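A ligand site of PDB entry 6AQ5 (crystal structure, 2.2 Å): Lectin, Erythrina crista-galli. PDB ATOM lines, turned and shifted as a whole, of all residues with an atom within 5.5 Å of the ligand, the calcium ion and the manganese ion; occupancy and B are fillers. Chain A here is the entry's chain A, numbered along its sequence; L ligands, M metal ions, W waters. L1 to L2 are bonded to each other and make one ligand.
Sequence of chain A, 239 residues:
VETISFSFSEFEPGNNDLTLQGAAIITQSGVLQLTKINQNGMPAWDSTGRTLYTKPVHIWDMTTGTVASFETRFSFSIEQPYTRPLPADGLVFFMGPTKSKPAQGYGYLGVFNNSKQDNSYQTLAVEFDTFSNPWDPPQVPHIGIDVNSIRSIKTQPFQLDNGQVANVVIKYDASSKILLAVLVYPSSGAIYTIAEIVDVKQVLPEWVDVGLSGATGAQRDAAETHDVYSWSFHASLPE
The manganese ion is bound by the side-chain carboxylate of Glu 127 (2.1 Å), the side-chain carboxylate of Asp 136 (2.2 Å), water W3 (2.2 Å), the side-chain carboxylate of Asp 129 (2.2 Å), a ring nitrogen (NE2) of His 142 (2.3 Å) and water W8 (2.3 Å). The manganese ion has six donor atoms within binding distance.
The calcium ion is bound by ND2 of Asn 133 (2.3 Å), OD2 of Asp 136 (2.3 Å), O of Phe 131 (2.3 Å), water W5 (2.4 Å), OD2 of Asp 129 (2.4 Å), water W7 (2.4 Å) and OD1 of Asp 129 (2.5 Å).
Along chain A the residues within 4 Å of the calcium ion span positions 129 to 136.
The nearest printed residue that does not touch the manganese ion is Ser 152 (4.2 Å).
OD1 of Asn 133 sits at hydrogen-bond distance from O2 of LG2 L2 (2.9 Å). The side-chain carboxylate (OD1) of Asp 89 sits at hydrogen-bond distance from an oxygen (O3) of LG2 L2 (2.6 Å). N of Gly 107 is in hydrogen-bond range of O2 of LG2 L2 (3.1 Å). An oxygen (O3) of LIG L1 sits at hydrogen-bond distance from the side-chain amide nitrogen of Gln 219, 3.1 Å away. The backbone NH (N) of Ala 218 is in hydrogen-bond range of an oxygen (O3) of LG2 L2 (3.3 Å).
N of Gly 107 lies within hydrogen-bond range of OD2 of Asp 89 (3.3 Å). The backbone carbonyl oxygen of Asp 89 is in hydrogen-bond range of the backbone NH of Thr 130 (3.0 Å). The backbone carbonyl oxygen (O) of Ala 222 sits at hydrogen-bond distance from the backbone NH (N) of Gly 217, 2.7 Å away.
CB of Ala 88 touches O3 of LG2 L2, 3.7 Å away. CB of Tyr 106 touches O2 of LG2 L2 (3.7 Å). CA of Gly 217 touches O3 of LG2 L2, at 3.2 Å. CB of Ala 222 touches O5 of LG2 L2 (3.6 Å). Ten residues have an atom within 4 Å of the ligand: Ala 88, Asp 89, Tyr 106, Gly 107, Phe 131, Asn 133, Gly 217, Ala 218, Gln 219 and Ala 222. The nearest printed residue that does not touch the ligand is Leu 86 (4.8 Å).
Water W8 bridges OE1 of Glu 127 and O of Ile 150. Water W9 bridges an oxygen (O5) of LG2 L2 (2.6 Å) and the backbone carbonyl oxygen (O) of Leu 86 (3.0 Å). Water W1 bridges an oxygen (O5) of LG2 L2 (2.7 Å) and the side-chain amide nitrogen (NE2) of Gln 219 (3.3 Å). Water W4 lies within hydrogen-bond range of an oxygen (O1) of LG2 L2 (2.8 Å) and the side-chain amide oxygen of Asn 133 (3.2 Å). Water W6 bridges O1 of LG2 L2 and N of Gly 107. Water W2 lies within hydrogen-bond range of O2 of LIG L1 and NE2 of Gln 219.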
ATOM      1  N   PRO A  85      -3.897  33.249  18.111  1.00  0.00           N
ATOM      2  CA  PRO A  85      -4.634  32.218  18.848  1.00  0.00           C
ATOM      3  C   PRO A  85      -3.962  31.859  20.167  1.00  0.00           C
ATOM      4  O   PRO A  85      -2.947  32.460  20.516  1.00  0.00           O
ATOM      5  CB  PRO A  85      -4.630  31.033  17.890  1.00  0.00           C
ATOM      6  CG  PRO A  85      -3.341  31.189  17.148  1.00  0.00           C
ATOM      7  CD  PRO A  85      -3.131  32.671  16.991  1.00  0.00           C
ATOM      8  N   LEU A  86      -4.524  30.888  20.883  1.00  0.00           N
ATOM      9  CA  LEU A  86      -3.933  30.454  22.132  1.00  0.00           C
ATOM     10  C   LEU A  86      -2.531  29.874  21.890  1.00  0.00           C
ATOM     11  O   LEU A  86      -2.279  29.271  20.839  1.00  0.00           O
ATOM     12  CB  LEU A  86      -4.822  29.400  22.805  1.00  0.00           C
ATOM     13  CG  LEU A  86      -6.224  29.853  23.216  1.00  0.00           C
ATOM     14  CD1 LEU A  86      -6.992  28.686  23.821  1.00  0.00           C
ATOM     15  CD2 LEU A  86      -6.172  31.013  24.199  1.00  0.00           C
ATOM     16  N   ALA A  88       0.772  27.306  22.428  1.00  0.00           N
ATOM     17  CA  ALA A  88       0.895  25.852  22.390  1.00  0.00           C
ATOM     18  C   ALA A  88       2.329  25.501  22.036  1.00  0.00           C
ATOM     19  O   ALA A  88       3.011  26.296  21.376  1.00  0.00           O
ATOM     20  CB  ALA A  88      -0.079  25.249  21.366  1.00  0.00           C
ATOM     21  N   ASP A  89       2.799  24.317  22.451  1.00  0.00           N
ATOM     22  CA  ASP A  89       2.050  23.333  23.232  1.00  0.00           C
ATOM     23  C   ASP A  89       2.715  23.042  24.588  1.00  0.00           C
ATOM     24  O   ASP A  89       2.040  22.619  25.525  1.00  0.00           O
ATOM     25  CB  ASP A  89       1.904  22.023  22.452  1.00  0.00           C
ATOM     26  CG  ASP A  89       0.629  21.973  21.614  1.00  0.00           C
ATOM     27  OD1 ASP A  89       0.717  22.225  20.395  1.00  0.00           O
ATOM     28  OD2 ASP A  89      -0.441  21.690  22.178  1.00  0.00           O
ATOM     29  N   TYR A 106       2.743  18.719  18.642  1.00  0.00           N
ATOM     30  CA  TYR A 106       1.548  19.387  19.186  1.00  0.00           C
ATOM     31  C   TYR A 106       1.392  18.949  20.649  1.00  0.00           C
ATOM     32  O   TYR A 106       2.393  18.886  21.366  1.00  0.00           O
ATOM     33  CB  TYR A 106       0.336  19.110  18.279  1.00  0.00           C
ATOM     34  CG  TYR A 106       0.584  19.358  16.808  1.00  0.00           C
ATOM     35  CD1 TYR A 106      -0.042  18.570  15.830  1.00  0.00           C
ATOM     36  CD2 TYR A 106       1.423  20.379  16.368  1.00  0.00           C
ATOM     37  CE1 TYR A 106       0.189  18.784  14.464  1.00  0.00           C
ATOM     38  CE2 TYR A 106       1.650  20.602  15.003  1.00  0.00           C
ATOM     39  CZ  TYR A 106       1.033  19.804  14.056  1.00  0.00           C
ATOM     40  OH  TYR A 106       1.238  20.018  12.717  1.00  0.00           O
ATOM     41  N   GLY A 107       0.176  18.615  21.106  1.00  0.00           N
ATOM     42  CA  GLY A 107      -0.048  18.296  22.501  1.00  0.00           C
ATOM     43  C   GLY A 107       0.561  16.987  22.951  1.00  0.00           C
ATOM     44  O   GLY A 107       0.495  16.680  24.146  1.00  0.00           O
ATOM     45  N   GLU A 127       5.767  17.155  32.603  1.00  0.00           N
ATOM     46  CA  GLU A 127       5.441  18.074  31.527  1.00  0.00           C
ATOM     47  C   GLU A 127       5.135  19.464  32.072  1.00  0.00           C
ATOM     48  O   GLU A 127       4.669  19.623  33.195  1.00  0.00           O
ATOM     49  CB  GLU A 127       4.250  17.575  30.709  1.00  0.00           C
ATOM     50  CG  GLU A 127       2.960  17.500  31.501  1.00  0.00           C
ATOM     51  CD  GLU A 127       1.736  17.268  30.638  1.00  0.00           C
ATOM     52  OE1 GLU A 127       1.788  16.411  29.734  1.00  0.00           O
ATOM     53  OE2 GLU A 127       0.721  17.956  30.844  1.00  0.00           O
ATOM     54  N   ASP A 129       2.887  22.136  30.449  1.00  0.00           N
ATOM     55  CA  ASP A 129       1.928  22.070  29.347  1.00  0.00           C
ATOM     56  C   ASP A 129       1.207  23.413  29.241  1.00  0.00           C
ATOM     57  O   ASP A 129       0.609  23.878  30.209  1.00  0.00           O
ATOM     58  CB  ASP A 129       0.949  20.922  29.600  1.00  0.00           C
ATOM     59  CG  ASP A 129       0.017  20.669  28.440  1.00  0.00           C
ATOM     60  OD1 ASP A 129      -0.027  21.471  27.480  1.00  0.00           O
ATOM     61  OD2 ASP A 129      -0.696  19.632  28.488  1.00  0.00           O
ATOM     62  N   THR A 130       1.244  24.016  28.046  1.00  0.00           N
ATOM     63  CA  THR A 130       0.701  25.350  27.851  1.00  0.00           C
ATOM     64  C   THR A 130      -0.605  25.401  27.071  1.00  0.00           C
ATOM     65  O   THR A 130      -1.190  26.484  26.953  1.00  0.00           O
ATOM     66  CB  THR A 130       1.745  26.235  27.139  1.00  0.00           C
ATOM     67  OG1 THR A 130       2.173  25.595  25.936  1.00  0.00           O
ATOM     68  CG2 THR A 130       2.954  26.460  28.040  1.00  0.00           C
ATOM     69  N   PHE A 131      -1.084  24.271  26.541  1.00  0.00           N
ATOM     70  CA  PHE A 131      -2.328  24.246  25.791  1.00  0.00           C
ATOM     71  C   PHE A 131      -3.240  23.143  26.313  1.00  0.00           C
ATOM     72  O   PHE A 131      -2.789  22.012  26.498  1.00  0.00           O
ATOM     73  CB  PHE A 131      -2.071  24.046  24.289  1.00  0.00           C
ATOM     74  CG  PHE A 131      -3.330  24.043  23.458  1.00  0.00           C
ATOM     75  CD1 PHE A 131      -3.812  25.211  22.897  1.00  0.00           C
ATOM     76  CD2 PHE A 131      -4.042  22.866  23.257  1.00  0.00           C
ATOM     77  CE1 PHE A 131      -4.980  25.211  22.150  1.00  0.00           C
ATOM     78  CE2 PHE A 131      -5.215  22.853  22.508  1.00  0.00           C
ATOM     79  CZ  PHE A 131      -5.679  24.028  21.950  1.00  0.00           C
ATOM     80  N   SER A 132      -4.507  23.474  26.534  1.00  0.00           N
ATOM     81  CA  SER A 132      -5.464  22.521  27.108  1.00  0.00           C
ATOM     82  C   SER A 132      -6.059  21.679  25.986  1.00  0.00           C
ATOM     83  O   SER A 132      -6.999  22.107  25.299  1.00  0.00           O
ATOM     84  CB  SER A 132      -6.537  23.243  27.899  1.00  0.00           C
ATOM     85  OG  SER A 132      -7.362  22.315  28.584  1.00  0.00           O
ATOM     86  N   ASN A 133      -5.515  20.489  25.791  1.00  0.00           N
ATOM     87  CA  ASN A 133      -6.045  19.508  24.855  1.00  0.00           C
ATOM     88  C   ASN A 133      -7.250  18.808  25.485  1.00  0.00           C
ATOM     89  O   ASN A 133      -7.514  18.964  26.676  1.00  0.00           O
ATOM     90  CB  ASN A 133      -4.948  18.510  24.493  1.00  0.00           C
ATOM     91  CG  ASN A 133      -3.839  19.120  23.657  1.00  0.00           C
ATOM     92  OD1 ASN A 133      -3.955  19.211  22.433  1.00  0.00           O
ATOM     93  ND2 ASN A 133      -2.759  19.520  24.306  1.00  0.00           N
ATOM     94  N   TRP A 135      -7.664  15.914  26.498  1.00  0.00           N
ATOM     95  CA  TRP A 135      -7.256  15.031  27.590  1.00  0.00           C
ATOM     96  C   TRP A 135      -6.653  15.775  28.783  1.00  0.00           C
ATOM     97  O   TRP A 135      -6.212  15.135  29.734  1.00  0.00           O
ATOM     98  CB  TRP A 135      -6.241  14.007  27.071  1.00  0.00           C
ATOM     99  CG  TRP A 135      -5.090  14.634  26.334  1.00  0.00           C
ATOM    100  CD1 TRP A 135      -3.959  15.164  26.883  1.00  0.00           C
ATOM    101  CD2 TRP A 135      -4.962  14.797  24.918  1.00  0.00           C
ATOM    102  NE1 TRP A 135      -3.136  15.648  25.903  1.00  0.00           N
ATOM    103  CE2 TRP A 135      -3.721  15.439  24.682  1.00  0.00           C
ATOM    104  CE3 TRP A 135      -5.766  14.476  23.817  1.00  0.00           C
ATOM    105  CZ2 TRP A 135      -3.269  15.751  23.398  1.00  0.00           C
ATOM    106  CZ3 TRP A 135      -5.316  14.786  22.543  1.00  0.00           C
ATOM    107  CH2 TRP A 135      -4.090  15.421  22.345  1.00  0.00           C
ATOM    108  N   ASP A 136      -6.621  17.116  28.748  1.00  0.00           N
ATOM    109  CA  ASP A 136      -5.984  17.960  29.744  1.00  0.00           C
ATOM    110  C   ASP A 136      -6.992  18.499  30.735  1.00  0.00           C
ATOM    111  O   ASP A 136      -8.202  18.546  30.465  1.00  0.00           O
ATOM    112  CB  ASP A 136      -5.294  19.149  29.059  1.00  0.00           C
ATOM    113  CG  ASP A 136      -3.946  18.785  28.489  1.00  0.00           C
ATOM    114  OD1 ASP A 136      -3.234  17.991  29.134  1.00  0.00           O
ATOM    115  OD2 ASP A 136      -3.603  19.300  27.406  1.00  0.00           O
ATOM    116  N   PRO A 137      -6.543  18.931  31.912  1.00  0.00           N
ATOM    117  CA  PRO A 137      -7.373  19.804  32.743  1.00  0.00           C
ATOM    118  C   PRO A 137      -7.622  21.121  32.038  1.00  0.00           C
ATOM    119  O   PRO A 137      -6.918  21.441  31.063  1.00  0.00           O
ATOM    120  CB  PRO A 137      -6.533  19.987  34.015  1.00  0.00           C
ATOM    121  CG  PRO A 137      -5.132  19.758  33.569  1.00  0.00           C
ATOM    122  CD  PRO A 137      -5.214  18.699  32.512  1.00  0.00           C
ATOM    123  N   HIS A 142       0.142  24.078  33.124  1.00  0.00           N
ATOM    124  CA  HIS A 142       0.108  23.184  34.276  1.00  0.00           C
ATOM    125  C   HIS A 142       1.306  22.271  34.222  1.00  0.00           C
ATOM    126  O   HIS A 142       1.803  21.919  33.142  1.00  0.00           O
ATOM    127  CB  HIS A 142      -1.197  22.365  34.341  1.00  0.00           C
ATOM    128  CG  HIS A 142      -1.460  21.533  33.123  1.00  0.00           C
ATOM    129  ND1 HIS A 142      -2.400  21.863  32.180  1.00  0.00           N
ATOM    130  CD2 HIS A 142      -0.905  20.362  32.708  1.00  0.00           C
ATOM    131  CE1 HIS A 142      -2.426  20.941  31.228  1.00  0.00           C
ATOM    132  NE2 HIS A 142      -1.521  20.024  31.529  1.00  0.00           N
ATOM    133  N   ILE A 150       0.197  10.766  27.713  1.00  0.00           N
ATOM    134  CA  ILE A 150       0.151  12.213  27.751  1.00  0.00           C
ATOM    135  C   ILE A 150      -0.928  12.690  28.716  1.00  0.00           C
ATOM    136  O   ILE A 150      -0.890  13.839  29.178  1.00  0.00           O
ATOM    137  CB  ILE A 150      -0.054  12.795  26.338  1.00  0.00           C
ATOM    138  CG1 ILE A 150       0.197  14.300  26.331  1.00  0.00           C
ATOM    139  CG2 ILE A 150      -1.455  12.490  25.839  1.00  0.00           C
ATOM    140  CD1 ILE A 150       1.618  14.708  26.652  1.00  0.00           C
ATOM    141  N   SER A 152      -1.995  13.032  32.084  1.00  0.00           N
ATOM    142  CA  SER A 152      -1.231  12.971  33.318  1.00  0.00           C
ATOM    143  C   SER A 152      -2.021  12.278  34.421  1.00  0.00           C
ATOM    144  O   SER A 152      -3.241  12.421  34.527  1.00  0.00           O
ATOM    145  CB  SER A 152      -0.863  14.387  33.784  1.00  0.00           C
ATOM    146  OG  SER A 152      -0.292  15.142  32.730  1.00  0.00           O
ATOM    147  N   THR A 155      -1.889  16.633  37.834  1.00  0.00           N
ATOM    148  CA  THR A 155      -1.564  17.938  37.266  1.00  0.00           C
ATOM    149  C   THR A 155      -1.624  19.003  38.335  1.00  0.00           C
ATOM    150  O   THR A 155      -2.362  18.882  39.328  1.00  0.00           O
ATOM    151  CB  THR A 155      -2.507  18.324  36.116  1.00  0.00           C
ATOM    152  OG1 THR A 155      -3.850  18.380  36.601  1.00  0.00           O
ATOM    153  CG2 THR A 155      -2.411  17.319  34.978  1.00  0.00           C
ATOM    154  N   THR A 216       5.515  23.383  19.400  1.00  0.00           N
ATOM    155  CA  THR A 216       4.540  24.433  19.145  1.00  0.00           C
ATOM    156  C   THR A 216       3.353  23.870  18.361  1.00  0.00           C
ATOM    157  O   THR A 216       3.365  22.737  17.887  1.00  0.00           O
ATOM    158  CB  THR A 216       5.179  25.610  18.402  1.00  0.00           C
ATOM    159  OG1 THR A 216       5.847  25.142  17.220  1.00  0.00           O
ATOM    160  CG2 THR A 216       6.197  26.310  19.301  1.00  0.00           C
ATOM    161  N   GLY A 217       2.319  24.702  18.225  1.00  0.00           N
ATOM    162  CA  GLY A 217       1.003  24.227  17.850  1.00  0.00           C
ATOM    163  C   GLY A 217       0.810  23.964  16.362  1.00  0.00           C
ATOM    164  O   GLY A 217       1.725  24.066  15.543  1.00  0.00           O
ATOM    165  N   ALA A 218      -0.437  23.624  16.022  1.00  0.00           N
ATOM    166  CA  ALA A 218      -0.800  23.092  14.713  1.00  0.00           C
ATOM    167  C   ALA A 218      -1.517  24.102  13.828  1.00  0.00           C
ATOM    168  O   ALA A 218      -2.046  23.720  12.779  1.00  0.00           O
ATOM    169  CB  ALA A 218      -1.658  21.842  14.880  1.00  0.00           C
ATOM    170  N   GLN A 219      -1.569  25.375  14.221  1.00  0.00           N
ATOM    171  CA  GLN A 219      -2.061  26.436  13.352  1.00  0.00           C
ATOM    172  C   GLN A 219      -1.194  27.663  13.550  1.00  0.00           C
ATOM    173  O   GLN A 219      -0.465  27.778  14.535  1.00  0.00           O
ATOM    174  CB  GLN A 219      -3.538  26.769  13.617  1.00  0.00           C
ATOM    175  CG  GLN A 219      -3.828  27.272  15.007  1.00  0.00           C
ATOM    176  CD  GLN A 219      -5.296  27.581  15.199  1.00  0.00           C
ATOM    177  OE1 GLN A 219      -5.709  28.745  15.175  1.00  0.00           O
ATOM    178  NE2 GLN A 219      -6.101  26.546  15.408  1.00  0.00           N
ATOM    179  N   ALA A 222       0.061  29.707  16.798  1.00  0.00           N
ATOM    180  CA  ALA A 222      -0.162  28.937  18.020  1.00  0.00           C
ATOM    181  C   ALA A 222       1.201  28.430  18.492  1.00  0.00           C
ATOM    182  O   ALA A 222       1.557  27.258  18.375  1.00  0.00           O
ATOM    183  CB  ALA A 222      -1.146  27.800  17.787  1.00  0.00           C
HETATM  184  C1  LIG L   1      -7.374  21.569  13.598  1.00  0.00           C
HETATM  185  C2  LIG L   1      -6.578  22.810  13.868  1.00  0.00           C
HETATM  186  C3  LIG L   1      -5.456  22.496  14.837  1.00  0.00           C
HETATM  187  C4  LIG L   1      -5.953  21.701  16.030  1.00  0.00           C
HETATM  188  C5  LIG L   1      -7.011  20.665  15.676  1.00  0.00           C
HETATM  189  C6  LIG L   1      -7.715  20.220  16.941  1.00  0.00           C
HETATM  190  O1  LIG L   1      -8.366  21.861  12.654  1.00  0.00           O
HETATM  191  O2  LIG L   1      -7.416  23.782  14.445  1.00  0.00           O
HETATM  192  O3  LIG L   1      -4.902  23.709  15.275  1.00  0.00           O
HETATM  193  O4  LIG L   1      -4.842  21.083  16.627  1.00  0.00           O
HETATM  194  O5  LIG L   1      -7.989  21.179  14.800  1.00  0.00           O
HETATM  195  O6  LIG L   1      -8.126  18.883  16.823  1.00  0.00           O
HETATM  196  C1  LG2 L   2      -4.546  21.573  17.911  1.00  0.00           C
HETATM  197  C2  LG2 L   2      -3.515  20.690  18.590  1.00  0.00           C
HETATM  198  C3  LG2 L   2      -3.187  21.270  19.950  1.00  0.00           C
HETATM  199  C4  LG2 L   2      -2.690  22.688  19.784  1.00  0.00           C
HETATM  200  C5  LG2 L   2      -3.701  23.519  19.021  1.00  0.00           C
HETATM  201  C6  LG2 L   2      -3.079  24.862  18.701  1.00  0.00           C
HETATM  202  O1  LG2 L   2      -4.017  19.387  18.758  1.00  0.00           O
HETATM  203  O2  LG2 L   2      -2.199  20.483  20.582  1.00  0.00           O
HETATM  204  O3  LG2 L   2      -1.474  22.692  19.065  1.00  0.00           O
HETATM  205  O4  LG2 L   2      -4.046  22.882  17.804  1.00  0.00           O
HETATM  206  O5  LG2 L   2      -4.055  25.731  18.161  1.00  0.00           O
HETATM  207 CA    CA M   1      -1.678  19.963  26.301  1.00  0.00          CA
HETATM  208 MN    MN M   2      -1.277  18.202  30.094  1.00  0.00          MN
HETATM  209  O   HOH W   1      -6.687  25.001  18.310  1.00  0.00           O
HETATM  210  O   HOH W   2      -8.978  25.387  16.470  1.00  0.00           O
HETATM  211  O   HOH W   3      -1.790  16.781  31.720  1.00  0.00           O
HETATM  212  O   HOH W   4      -6.255  18.908  20.299  1.00  0.00           O
HETATM  213  O   HOH W   5      -0.143  20.842  24.660  1.00  0.00           O
HETATM  214  O   HOH W   6      -2.296  17.318  19.871  1.00  0.00           O
HETATM  215  O   HOH W   7      -0.877  17.697  25.956  1.00  0.00           O
HETATM  216  O   HOH W   8      -0.507  16.463  28.719  1.00  0.00           O
HETATM  217  O   HOH W   9      -4.509  27.931  19.388  1.00  0.00           O
HETATM  218  O   HOH W  10      -8.176  16.953  19.286  1.00  0.00           O
